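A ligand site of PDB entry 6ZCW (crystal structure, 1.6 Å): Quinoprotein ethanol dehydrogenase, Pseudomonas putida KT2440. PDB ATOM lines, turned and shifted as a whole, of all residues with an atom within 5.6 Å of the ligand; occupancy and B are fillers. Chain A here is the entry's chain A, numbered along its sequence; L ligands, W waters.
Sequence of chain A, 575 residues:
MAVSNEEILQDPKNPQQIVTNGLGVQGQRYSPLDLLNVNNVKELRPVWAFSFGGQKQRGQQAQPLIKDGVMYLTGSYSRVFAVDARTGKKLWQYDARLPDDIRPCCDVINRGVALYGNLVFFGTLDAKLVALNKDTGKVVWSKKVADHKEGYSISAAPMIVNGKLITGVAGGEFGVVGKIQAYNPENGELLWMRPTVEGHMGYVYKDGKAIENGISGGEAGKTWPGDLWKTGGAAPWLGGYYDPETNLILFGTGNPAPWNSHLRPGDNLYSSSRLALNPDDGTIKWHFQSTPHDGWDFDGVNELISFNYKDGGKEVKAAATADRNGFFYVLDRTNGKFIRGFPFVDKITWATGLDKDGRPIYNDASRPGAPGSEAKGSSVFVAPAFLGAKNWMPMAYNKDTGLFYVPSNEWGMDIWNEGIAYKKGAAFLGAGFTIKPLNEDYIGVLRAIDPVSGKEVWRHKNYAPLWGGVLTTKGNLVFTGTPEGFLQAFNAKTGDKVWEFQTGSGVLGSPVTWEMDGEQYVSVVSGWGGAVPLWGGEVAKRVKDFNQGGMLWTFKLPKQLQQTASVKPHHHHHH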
ATOM      1  N   GLN A  61     -19.945 -14.568  -7.672  1.00  0.00           N
ATOM      2  CA  GLN A  61     -21.109 -15.233  -7.086  1.00  0.00           C
ATOM      3  C   GLN A  61     -21.517 -14.731  -5.715  1.00  0.00           C
ATOM      4  O   GLN A  61     -22.447 -15.290  -5.131  1.00  0.00           O
ATOM      5  CB  GLN A  61     -20.842 -16.746  -6.999  1.00  0.00           C
ATOM      6  CG  GLN A  61     -20.754 -17.433  -8.362  1.00  0.00           C
ATOM      7  CD  GLN A  61     -20.581 -18.942  -8.267  1.00  0.00           C
ATOM      8  OE1 GLN A  61     -20.560 -19.513  -7.174  1.00  0.00           O
ATOM      9  NE2 GLN A  61     -20.451 -19.592  -9.419  1.00  0.00           N
ATOM     10  N   CYS A 105     -12.028 -26.496  -9.218  1.00  0.00           N
ATOM     11  CA  CYS A 105     -12.508 -27.218 -10.391  1.00  0.00           C
ATOM     12  C   CYS A 105     -13.198 -26.303 -11.393  1.00  0.00           C
ATOM     13  O   CYS A 105     -13.184 -26.571 -12.601  1.00  0.00           O
ATOM     14  CB  CYS A 105     -13.485 -28.326  -9.994  1.00  0.00           C
ATOM     15  SG  CYS A 105     -15.088 -27.705  -9.318  1.00  0.00           S
ATOM     16  N   CYS A 106     -13.857 -25.270 -10.895  1.00  0.00           N
ATOM     17  CA  CYS A 106     -15.017 -24.691 -11.585  1.00  0.00           C
ATOM     18  C   CYS A 106     -15.048 -23.174 -11.465  1.00  0.00           C
ATOM     19  O   CYS A 106     -16.087 -22.577 -11.184  1.00  0.00           O
ATOM     20  CB  CYS A 106     -16.294 -25.302 -11.028  1.00  0.00           C
ATOM     21  SG  CYS A 106     -16.254 -27.128 -10.928  1.00  0.00           S
ATOM     22  N   ILE A 109     -14.298 -18.658  -8.044  1.00  0.00           N
ATOM     23  CA  ILE A 109     -15.459 -17.967  -7.499  1.00  0.00           C
ATOM     24  C   ILE A 109     -15.419 -17.981  -5.976  1.00  0.00           C
ATOM     25  O   ILE A 109     -14.753 -18.804  -5.345  1.00  0.00           O
ATOM     26  CB  ILE A 109     -16.754 -18.588  -8.032  1.00  0.00           C
ATOM     27  CG1 ILE A 109     -16.668 -20.109  -7.975  1.00  0.00           C
ATOM     28  CG2 ILE A 109     -16.904 -18.305  -9.509  1.00  0.00           C
ATOM     29  CD1 ILE A 109     -17.098 -20.671  -6.737  1.00  0.00           C
ATOM     30  N   ARG A 111     -18.523 -17.142  -2.704  1.00  0.00           N
ATOM     31  CA  ARG A 111     -19.944 -16.877  -2.557  1.00  0.00           C
ATOM     32  C   ARG A 111     -20.287 -15.935  -1.418  1.00  0.00           C
ATOM     33  O   ARG A 111     -21.472 -15.642  -1.224  1.00  0.00           O
ATOM     34  CB  ARG A 111     -20.697 -18.206  -2.418  1.00  0.00           C
ATOM     35  CG  ARG A 111     -20.451 -19.093  -3.648  1.00  0.00           C
ATOM     36  CD  ARG A 111     -21.287 -20.372  -3.716  1.00  0.00           C
ATOM     37  NE  ARG A 111     -20.797 -21.090  -4.898  1.00  0.00           N
ATOM     38  CZ  ARG A 111     -19.864 -22.032  -4.868  1.00  0.00           C
ATOM     39  NH1 ARG A 111     -19.377 -22.469  -3.698  1.00  0.00           N
ATOM     40  NH2 ARG A 111     -19.442 -22.563  -6.016  1.00  0.00           N
ATOM     41  N   SER A 153      -9.926 -26.422  -1.937  1.00  0.00           N
ATOM     42  CA  SER A 153     -10.154 -24.985  -2.024  1.00  0.00           C
ATOM     43  C   SER A 153     -11.368 -24.687  -1.171  1.00  0.00           C
ATOM     44  O   SER A 153     -12.026 -25.586  -0.648  1.00  0.00           O
ATOM     45  CB  SER A 153     -10.355 -24.534  -3.494  1.00  0.00           C
ATOM     46  OG  SER A 153     -11.487 -25.183  -4.041  1.00  0.00           O
ATOM     47  N   SER A 155     -14.837 -22.230  -1.718  1.00  0.00           N
ATOM     48  CA  SER A 155     -15.613 -21.334  -2.551  1.00  0.00           C
ATOM     49  C   SER A 155     -16.872 -20.815  -1.873  1.00  0.00           C
ATOM     50  O   SER A 155     -17.431 -19.816  -2.343  1.00  0.00           O
ATOM     51  CB  SER A 155     -16.009 -22.046  -3.865  1.00  0.00           C
ATOM     52  OG  SER A 155     -16.686 -23.270  -3.608  1.00  0.00           O
ATOM     53  N   VAL A 169     -15.290 -27.371   2.697  1.00  0.00           N
ATOM     54  CA  VAL A 169     -14.191 -27.313   1.737  1.00  0.00           C
ATOM     55  C   VAL A 169     -14.700 -27.847   0.410  1.00  0.00           C
ATOM     56  O   VAL A 169     -15.747 -28.494   0.338  1.00  0.00           O
ATOM     57  CB  VAL A 169     -12.938 -28.123   2.162  1.00  0.00           C
ATOM     58  CG1 VAL A 169     -12.243 -27.496   3.377  1.00  0.00           C
ATOM     59  CG2 VAL A 169     -13.297 -29.590   2.399  1.00  0.00           C
ATOM     60  N   ALA A 170     -13.927 -27.590  -0.646  1.00  0.00           N
ATOM     61  CA  ALA A 170     -14.225 -27.993  -2.010  1.00  0.00           C
ATOM     62  C   ALA A 170     -13.087 -28.852  -2.554  1.00  0.00           C
ATOM     63  O   ALA A 170     -11.949 -28.758  -2.091  1.00  0.00           O
ATOM     64  CB  ALA A 170     -14.413 -26.759  -2.909  1.00  0.00           C
ATOM     65  N   GLY A 171     -13.396 -29.673  -3.564  1.00  0.00           N
ATOM     66  CA  GLY A 171     -12.344 -30.409  -4.241  1.00  0.00           C
ATOM     67  C   GLY A 171     -12.635 -31.855  -4.602  1.00  0.00           C
ATOM     68  O   GLY A 171     -11.702 -32.629  -4.855  1.00  0.00           O
ATOM     69  N   GLY A 172     -13.914 -32.244  -4.626  1.00  0.00           N
ATOM     70  CA  GLY A 172     -14.233 -33.630  -4.959  1.00  0.00           C
ATOM     71  C   GLY A 172     -13.693 -34.094  -6.303  1.00  0.00           C
ATOM     72  O   GLY A 172     -13.355 -35.265  -6.477  1.00  0.00           O
ATOM     73  N   GLU A 173     -13.600 -33.182  -7.280  1.00  0.00           N
ATOM     74  CA  GLU A 173     -13.035 -33.559  -8.565  1.00  0.00           C
ATOM     75  C   GLU A 173     -11.556 -33.868  -8.473  1.00  0.00           C
ATOM     76  O   GLU A 173     -10.982 -34.378  -9.443  1.00  0.00           O
ATOM     77  CB  GLU A 173     -13.291 -32.452  -9.609  1.00  0.00           C
ATOM     78  CG  GLU A 173     -14.631 -32.571 -10.359  1.00  0.00           C
ATOM     79  CD  GLU A 173     -15.842 -32.442  -9.441  1.00  0.00           C
ATOM     80  OE1 GLU A 173     -16.194 -31.306  -9.049  1.00  0.00           O
ATOM     81  OE2 GLU A 173     -16.473 -33.463  -9.101  1.00  0.00           O
ATOM     82  N   ALA A 235     -17.310 -33.469  -1.002  1.00  0.00           N
ATOM     83  CA  ALA A 235     -16.888 -32.187  -0.435  1.00  0.00           C
ATOM     84  C   ALA A 235     -18.113 -31.333  -0.136  1.00  0.00           C
ATOM     85  O   ALA A 235     -18.990 -31.180  -0.986  1.00  0.00           O
ATOM     86  CB  ALA A 235     -15.952 -31.442  -1.392  1.00  0.00           C
ATOM     87  N   TRP A 237     -19.065 -28.263  -0.363  1.00  0.00           N
ATOM     88  CA  TRP A 237     -18.431 -27.098  -0.973  1.00  0.00           C
ATOM     89  C   TRP A 237     -19.359 -25.904  -1.125  1.00  0.00           C
ATOM     90  O   TRP A 237     -18.870 -24.833  -1.508  1.00  0.00           O
ATOM     91  CB  TRP A 237     -17.887 -27.478  -2.343  1.00  0.00           C
ATOM     92  CG  TRP A 237     -18.846 -28.082  -3.362  1.00  0.00           C
ATOM     93  CD1 TRP A 237     -19.040 -29.416  -3.613  1.00  0.00           C
ATOM     94  CD2 TRP A 237     -19.667 -27.384  -4.297  1.00  0.00           C
ATOM     95  NE1 TRP A 237     -19.936 -29.579  -4.653  1.00  0.00           N
ATOM     96  CE2 TRP A 237     -20.331 -28.335  -5.076  1.00  0.00           C
ATOM     97  CE3 TRP A 237     -19.893 -26.018  -4.542  1.00  0.00           C
ATOM     98  CZ2 TRP A 237     -21.214 -27.987  -6.119  1.00  0.00           C
ATOM     99  CZ3 TRP A 237     -20.788 -25.666  -5.573  1.00  0.00           C
ATOM    100  CH2 TRP A 237     -21.425 -26.643  -6.348  1.00  0.00           C
ATOM    101  N   GLY A 254     -20.770 -33.142  -1.646  1.00  0.00           N
ATOM    102  CA  GLY A 254     -20.474 -33.285  -3.059  1.00  0.00           C
ATOM    103  C   GLY A 254     -20.525 -34.724  -3.556  1.00  0.00           C
ATOM    104  O   GLY A 254     -20.761 -35.673  -2.804  1.00  0.00           O
ATOM    105  N   ASN A 255     -20.316 -34.859  -4.854  1.00  0.00           N
ATOM    106  CA  ASN A 255     -20.267 -36.178  -5.489  1.00  0.00           C
ATOM    107  C   ASN A 255     -19.154 -37.042  -4.896  1.00  0.00           C
ATOM    108  O   ASN A 255     -18.139 -36.524  -4.414  1.00  0.00           O
ATOM    109  CB  ASN A 255     -20.024 -36.022  -6.980  1.00  0.00           C
ATOM    110  CG  ASN A 255     -18.719 -35.336  -7.284  1.00  0.00           C
ATOM    111  OD1 ASN A 255     -18.519 -34.162  -6.924  1.00  0.00           O
ATOM    112  ND2 ASN A 255     -17.809 -36.055  -7.929  1.00  0.00           N
ATOM    113  N   ASP A 297     -21.725 -37.295 -11.327  1.00  0.00           N
ATOM    114  CA  ASP A 297     -21.336 -36.049 -10.668  1.00  0.00           C
ATOM    115  C   ASP A 297     -22.572 -35.242 -10.258  1.00  0.00           C
ATOM    116  O   ASP A 297     -22.607 -34.009 -10.348  1.00  0.00           O
ATOM    117  CB  ASP A 297     -20.386 -35.251 -11.577  1.00  0.00           C
ATOM    118  CG  ASP A 297     -19.962 -33.897 -10.999  1.00  0.00           C
ATOM    119  OD1 ASP A 297     -19.445 -33.828  -9.874  1.00  0.00           O
ATOM    120  OD2 ASP A 297     -20.134 -32.889 -11.736  1.00  0.00           O
ATOM    121  N   ASP A 299     -23.615 -33.938  -7.498  1.00  0.00           N
ATOM    122  CA  ASP A 299     -23.330 -33.474  -6.137  1.00  0.00           C
ATOM    123  C   ASP A 299     -24.626 -33.271  -5.367  1.00  0.00           C
ATOM    124  O   ASP A 299     -25.648 -32.855  -5.924  1.00  0.00           O
ATOM    125  CB  ASP A 299     -22.559 -32.145  -6.150  1.00  0.00           C
ATOM    126  CG  ASP A 299     -21.194 -32.261  -6.787  1.00  0.00           C
ATOM    127  OD1 ASP A 299     -21.113 -32.645  -7.976  1.00  0.00           O
ATOM    128  OD2 ASP A 299     -20.191 -31.909  -6.115  1.00  0.00           O
ATOM    129  N   ARG A 324     -29.249 -31.482  -7.888  1.00  0.00           N
ATOM    130  CA  ARG A 324     -28.577 -31.659  -9.173  1.00  0.00           C
ATOM    131  C   ARG A 324     -29.220 -32.760 -10.006  1.00  0.00           C
ATOM    132  O   ARG A 324     -29.267 -32.670 -11.244  1.00  0.00           O
ATOM    133  CB  ARG A 324     -27.085 -31.994  -8.941  1.00  0.00           C
ATOM    134  CG  ARG A 324     -26.237 -30.860  -8.363  1.00  0.00           C
ATOM    135  CD  ARG A 324     -25.575 -30.024  -9.479  1.00  0.00           C
ATOM    136  NE  ARG A 324     -24.463 -30.719 -10.131  1.00  0.00           N
ATOM    137  CZ  ARG A 324     -23.184 -30.568  -9.771  1.00  0.00           C
ATOM    138  NH1 ARG A 324     -22.870 -29.766  -8.767  1.00  0.00           N
ATOM    139  NH2 ARG A 324     -22.225 -31.227 -10.428  1.00  0.00           N
ATOM    140  N   PHE A 386     -24.389 -33.396 -15.928  1.00  0.00           N
ATOM    141  CA  PHE A 386     -23.747 -33.371 -14.614  1.00  0.00           C
ATOM    142  C   PHE A 386     -23.830 -32.002 -13.964  1.00  0.00           C
ATOM    143  O   PHE A 386     -23.948 -31.920 -12.732  1.00  0.00           O
ATOM    144  CB  PHE A 386     -22.289 -33.853 -14.720  1.00  0.00           C
ATOM    145  CG  PHE A 386     -21.378 -32.969 -15.552  1.00  0.00           C
ATOM    146  CD1 PHE A 386     -20.739 -31.868 -14.980  1.00  0.00           C
ATOM    147  CD2 PHE A 386     -21.079 -33.302 -16.865  1.00  0.00           C
ATOM    148  CE1 PHE A 386     -19.884 -31.084 -15.740  1.00  0.00           C
ATOM    149  CE2 PHE A 386     -20.235 -32.523 -17.616  1.00  0.00           C
ATOM    150  CZ  PHE A 386     -19.626 -31.417 -17.054  1.00  0.00           C
ATOM    151  N   LEU A 387     -23.830 -30.914 -14.745  1.00  0.00           N
ATOM    152  CA  LEU A 387     -23.999 -29.593 -14.155  1.00  0.00           C
ATOM    153  C   LEU A 387     -25.371 -29.407 -13.507  1.00  0.00           C
ATOM    154  O   LEU A 387     -25.555 -28.437 -12.762  1.00  0.00           O
ATOM    155  CB  LEU A 387     -23.743 -28.507 -15.209  1.00  0.00           C
ATOM    156  CG  LEU A 387     -22.275 -28.328 -15.618  1.00  0.00           C
ATOM    157  CD1 LEU A 387     -22.155 -27.177 -16.615  1.00  0.00           C
ATOM    158  CD2 LEU A 387     -21.346 -28.121 -14.407  1.00  0.00           C
ATOM    159  N   ASN A 391     -27.667 -26.108 -10.001  1.00  0.00           N
ATOM    160  CA  ASN A 391     -26.312 -26.181  -9.466  1.00  0.00           C
ATOM    161  C   ASN A 391     -26.210 -25.344  -8.187  1.00  0.00           C
ATOM    162  O   ASN A 391     -27.118 -25.367  -7.357  1.00  0.00           O
ATOM    163  CB  ASN A 391     -25.309 -25.748 -10.545  1.00  0.00           C
ATOM    164  CG  ASN A 391     -23.911 -26.264 -10.298  1.00  0.00           C
ATOM    165  OD1 ASN A 391     -23.185 -25.734  -9.456  1.00  0.00           O
ATOM    166  ND2 ASN A 391     -23.517 -27.301 -11.025  1.00  0.00           N
ATOM    167  N   TRP A 392     -25.112 -24.603  -8.021  1.00  0.00           N
ATOM    168  CA  TRP A 392     -24.821 -23.902  -6.766  1.00  0.00           C
ATOM    169  C   TRP A 392     -25.889 -22.852  -6.444  1.00  0.00           C
ATOM    170  O   TRP A 392     -26.101 -22.521  -5.265  1.00  0.00           O
ATOM    171  CB  TRP A 392     -23.457 -23.207  -6.867  1.00  0.00           C
ATOM    172  CG  TRP A 392     -23.599 -21.945  -7.672  1.00  0.00           C
ATOM    173  CD1 TRP A 392     -23.588 -21.827  -9.026  1.00  0.00           C
ATOM    174  CD2 TRP A 392     -23.891 -20.637  -7.153  1.00  0.00           C
ATOM    175  NE1 TRP A 392     -23.840 -20.518  -9.393  1.00  0.00           N
ATOM    176  CE2 TRP A 392     -24.022 -19.767  -8.264  1.00  0.00           C
ATOM    177  CE3 TRP A 392     -24.048 -20.109  -5.861  1.00  0.00           C
ATOM    178  CZ2 TRP A 392     -24.298 -18.410  -8.116  1.00  0.00           C
ATOM    179  CZ3 TRP A 392     -24.311 -18.760  -5.715  1.00  0.00           C
ATOM    180  CH2 TRP A 392     -24.442 -17.929  -6.838  1.00  0.00           C
ATOM    181  N   TRP A 467     -27.742 -19.294 -13.962  1.00  0.00           N
ATOM    182  CA  TRP A 467     -26.619 -19.626 -13.084  1.00  0.00           C
ATOM    183  C   TRP A 467     -26.544 -18.691 -11.870  1.00  0.00           C
ATOM    184  O   TRP A 467     -25.477 -18.583 -11.259  1.00  0.00           O
ATOM    185  CB  TRP A 467     -25.278 -19.620 -13.862  1.00  0.00           C
ATOM    186  CG  TRP A 467     -24.269 -20.622 -13.336  1.00  0.00           C
ATOM    187  CD1 TRP A 467     -23.150 -20.357 -12.592  1.00  0.00           C
ATOM    188  CD2 TRP A 467     -24.317 -22.051 -13.496  1.00  0.00           C
ATOM    189  NE1 TRP A 467     -22.501 -21.531 -12.286  1.00  0.00           N
ATOM    190  CE2 TRP A 467     -23.194 -22.589 -12.836  1.00  0.00           C
ATOM    191  CE3 TRP A 467     -25.198 -22.921 -14.163  1.00  0.00           C
ATOM    192  CZ2 TRP A 467     -22.926 -23.960 -12.790  1.00  0.00           C
ATOM    193  CZ3 TRP A 467     -24.929 -24.292 -14.117  1.00  0.00           C
ATOM    194  CH2 TRP A 467     -23.805 -24.803 -13.439  1.00  0.00           C
ATOM    195  N   GLY A 529     -19.326 -16.148 -15.325  1.00  0.00           N
ATOM    196  CA  GLY A 529     -18.335 -17.174 -15.067  1.00  0.00           C
ATOM    197  C   GLY A 529     -18.968 -18.397 -14.443  1.00  0.00           C
ATOM    198  O   GLY A 529     -20.145 -18.684 -14.684  1.00  0.00           O
ATOM    199  N   GLY A 530     -18.187 -19.093 -13.623  1.00  0.00           N
ATOM    200  CA  GLY A 530     -18.626 -20.362 -13.069  1.00  0.00           C
ATOM    201  C   GLY A 530     -18.247 -21.512 -13.977  1.00  0.00           C
ATOM    202  O   GLY A 530     -17.410 -21.382 -14.871  1.00  0.00           O
ATOM    203  N   ALA A 531     -18.918 -22.656 -13.768  1.00  0.00           N
ATOM    204  CA  ALA A 531     -18.522 -23.887 -14.459  1.00  0.00           C
ATOM    205  C   ALA A 531     -18.869 -23.900 -15.948  1.00  0.00           C
ATOM    206  O   ALA A 531     -18.223 -24.634 -16.711  1.00  0.00           O
ATOM    207  CB  ALA A 531     -19.174 -25.095 -13.790  1.00  0.00           C
ATOM    208  N   VAL A 532     -19.894 -23.174 -16.391  1.00  0.00           N
ATOM    209  CA  VAL A 532     -20.411 -23.400 -17.751  1.00  0.00           C
ATOM    210  C   VAL A 532     -19.367 -23.136 -18.838  1.00  0.00           C
ATOM    211  O   VAL A 532     -19.252 -23.955 -19.760  1.00  0.00           O
ATOM    212  CB  VAL A 532     -21.704 -22.595 -17.970  1.00  0.00           C
ATOM    213  CG1 VAL A 532     -22.051 -22.567 -19.457  1.00  0.00           C
ATOM    214  CG2 VAL A 532     -22.846 -23.230 -17.175  1.00  0.00           C
HETATM  215  N1  LIG L   1     -18.828 -24.933  -8.683  1.00  0.00           N
HETATM  216  C1  LIG L   1     -19.586 -24.495  -9.736  1.00  0.00           C
HETATM  217  C2  LIG L   1     -19.778 -23.027 -10.043  1.00  0.00           C
HETATM  218  O1  LIG L   1     -19.527 -22.236  -9.097  1.00  0.00           O
HETATM  219  O2  LIG L   1     -20.214 -22.657 -11.158  1.00  0.00           O
HETATM  220  C3  LIG L   1     -20.139 -25.562 -10.421  1.00  0.00           C
HETATM  221  C4  LIG L   1     -19.724 -26.681  -9.782  1.00  0.00           C
HETATM  222  C5  LIG L   1     -18.897 -26.292  -8.697  1.00  0.00           C
HETATM  223  C6  LIG L   1     -19.991 -28.134 -10.061  1.00  0.00           C
HETATM  224  O3  LIG L   1     -20.689 -28.437 -10.990  1.00  0.00           O
HETATM  225  C7  LIG L   1     -19.393 -29.118  -9.198  1.00  0.00           C
HETATM  226  O4  LIG L   1     -19.564 -30.293  -9.348  1.00  0.00           O
HETATM  227  C8  LIG L   1     -18.519 -28.687  -8.067  1.00  0.00           C
HETATM  228  N2  LIG L   1     -17.951 -29.649  -7.272  1.00  0.00           N
HETATM  229  C9  LIG L   1     -17.161 -29.255  -6.239  1.00  0.00           C
HETATM  230  C10 LIG L   1     -16.740 -30.543  -5.567  1.00  0.00           C
HETATM  231  O5  LIG L   1     -15.959 -30.436  -4.589  1.00  0.00           O
HETATM  232  O6  LIG L   1     -17.167 -31.658  -5.969  1.00  0.00           O
HETATM  233  C11 LIG L   1     -16.913 -27.889  -5.976  1.00  0.00           C
HETATM  234  C12 LIG L   1     -17.478 -26.933  -6.784  1.00  0.00           C
HETATM  235  C13 LIG L   1     -16.974 -25.639  -6.148  1.00  0.00           C
HETATM  236  O7  LIG L   1     -16.205 -25.613  -5.164  1.00  0.00           O
HETATM  237  O8  LIG L   1     -17.415 -24.546  -6.576  1.00  0.00           O
HETATM  238  C14 LIG L   1     -18.278 -27.329  -7.818  1.00  0.00           C
HETATM  239  O   HOH W   1     -19.436 -30.615 -12.105  1.00  0.00           O
HETATM  240  O   HOH W   2     -14.079 -30.200  -7.287  1.00  0.00           O
HETATM  241  O   HOH W   3     -17.314 -33.688  -4.014  1.00  0.00           O
HETATM  242  O   HOH W   4     -13.786 -24.743  -5.667  1.00  0.00           O
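Water W4 lies within hydrogen-bond range of an oxygen (O7) of the ligand (2.6 Å) and the side-chain hydroxyl (OG) of Ser 153 (2.9 Å). Water W1 lies within hydrogen-bond range of the side-chain carboxylate (OD2) of Asp 297 (2.4 Å), an oxygen (O3) of the ligand (2.7 Å) and the guanidinium group (NH2) of Arg 324 (3.3 Å). Water W3 lies within hydrogen-bond range of an oxygen (O6) of the ligand, the backbone carbonyl oxygen (O) of Asn 255 and the backbone NH (N) of Ala 235. Water W2 lies within hydrogen-bond range of the side-chain carboxylate of Glu 173 (3.0 Å), an oxygen (O5) of the ligand (3.3 Å), the backbone NH of Gly 172 (3.4 Å) and the side-chain sulfur of Cys 105 (3.4 Å).
The backbone NH (N) of Gly 172 lies within hydrogen-bond range of an oxygen (O5) of the ligand, 2.7 Å away. O2 of the ligand lies within hydrogen-bond range of NE1 of Trp 467 (2.8 Å). O1 of the ligand is in hydrogen-bond range of NE2 of Gln 61. The side-chain hydroxyl (OG) of Ser 155 sits at hydrogen-bond distance from an oxygen (O7) of the ligand (2.9 Å). N of Gly 171 sits at hydrogen-bond distance from O5 of the ligand (2.9 Å). O8 of the ligand lies within salt-bridge range of NH2 of Arg 111 (2.9 Å). N of Ala 531 sits at hydrogen-bond distance from O2 of the ligand (2.9 Å). An oxygen (O6) of the ligand lies close to the side-chain amide oxygen (OD1) of Asn 255. NH2 of Arg 324 lies within hydrogen-bond range of O4 of the ligand (3.0 Å). OD2 of Asp 299 lies close to O6 of the ligand (3.0 Å). O3 of the ligand lies within hydrogen-bond range of ND2 of Asn 391, at 3.0 Å. NE1 of Trp 237 lies close to N2 of the ligand (3.3 Å).
A nitrogen (N2) of the ligand lies close to the side-chain carboxylate (OE1) of Glu 173 (3.0 Å). Residues that only touch the ligand: Ala 170 (3.1 Å), Ala 235 (3.4 Å), Gly 530 (3.4 Å), Cys 106 (3.5 Å), Leu 387 (3.5 Å), Cys 105 (3.5 Å), Asp 297 (3.6 Å) and Ile 109 (3.7 Å). Hydrophobic or aromatic side chains within 4 Å of the ligand: Ile 109, Ala 170, Ala 235, Trp 237, Leu 387, Trp 467 and Ala 531. Within 4 Å of the ligand: Gln 61, Cys 105, Cys 106, Ile 109, Arg 111, Ser 155, Ala 170, Gly 171, Gly 172, Glu 173, Ala 235, Trp 237, Asn 255, Asp 297, Asp 299, Arg 324, Leu 387, Asn 391, Trp 467, Gly 530 and Ala 531.
OE2 of Glu 173 sits close to OD1 of Asn 255. OD1 of Asn 255 lies close to OD2 of Asp 299 (2.9 Å). The guanidinium group (NH2) of Arg 324 is in salt-bridge range of the side-chain carboxylate (OD1) of Asp 299 (3.0 Å). The side-chain amide nitrogen (ND2) of Asn 391 sits close to the guanidinium group (NH1) of Arg 324, at 3.4 Å. The indole nitrogen (NE1) of Trp 237 lies within hydrogen-bond range of the side-chain carboxylate (OD2) of Asp 299 (2.8 Å). The backbone carbonyl oxygen (O) of Leu 387 lies within hydrogen-bond range of the side-chain amide nitrogen (ND2) of Asn 391, 2.9 Å away. The backbone NH (N) of Gly 254 lies within hydrogen-bond range of the backbone carbonyl oxygen (O) of Ala 235, at 2.7 Å. The side-chain sulfur (SG) of Cys 105 forms a disulfide with the side-chain sulfur (SG) of Cys 106, 2.1 Å away.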
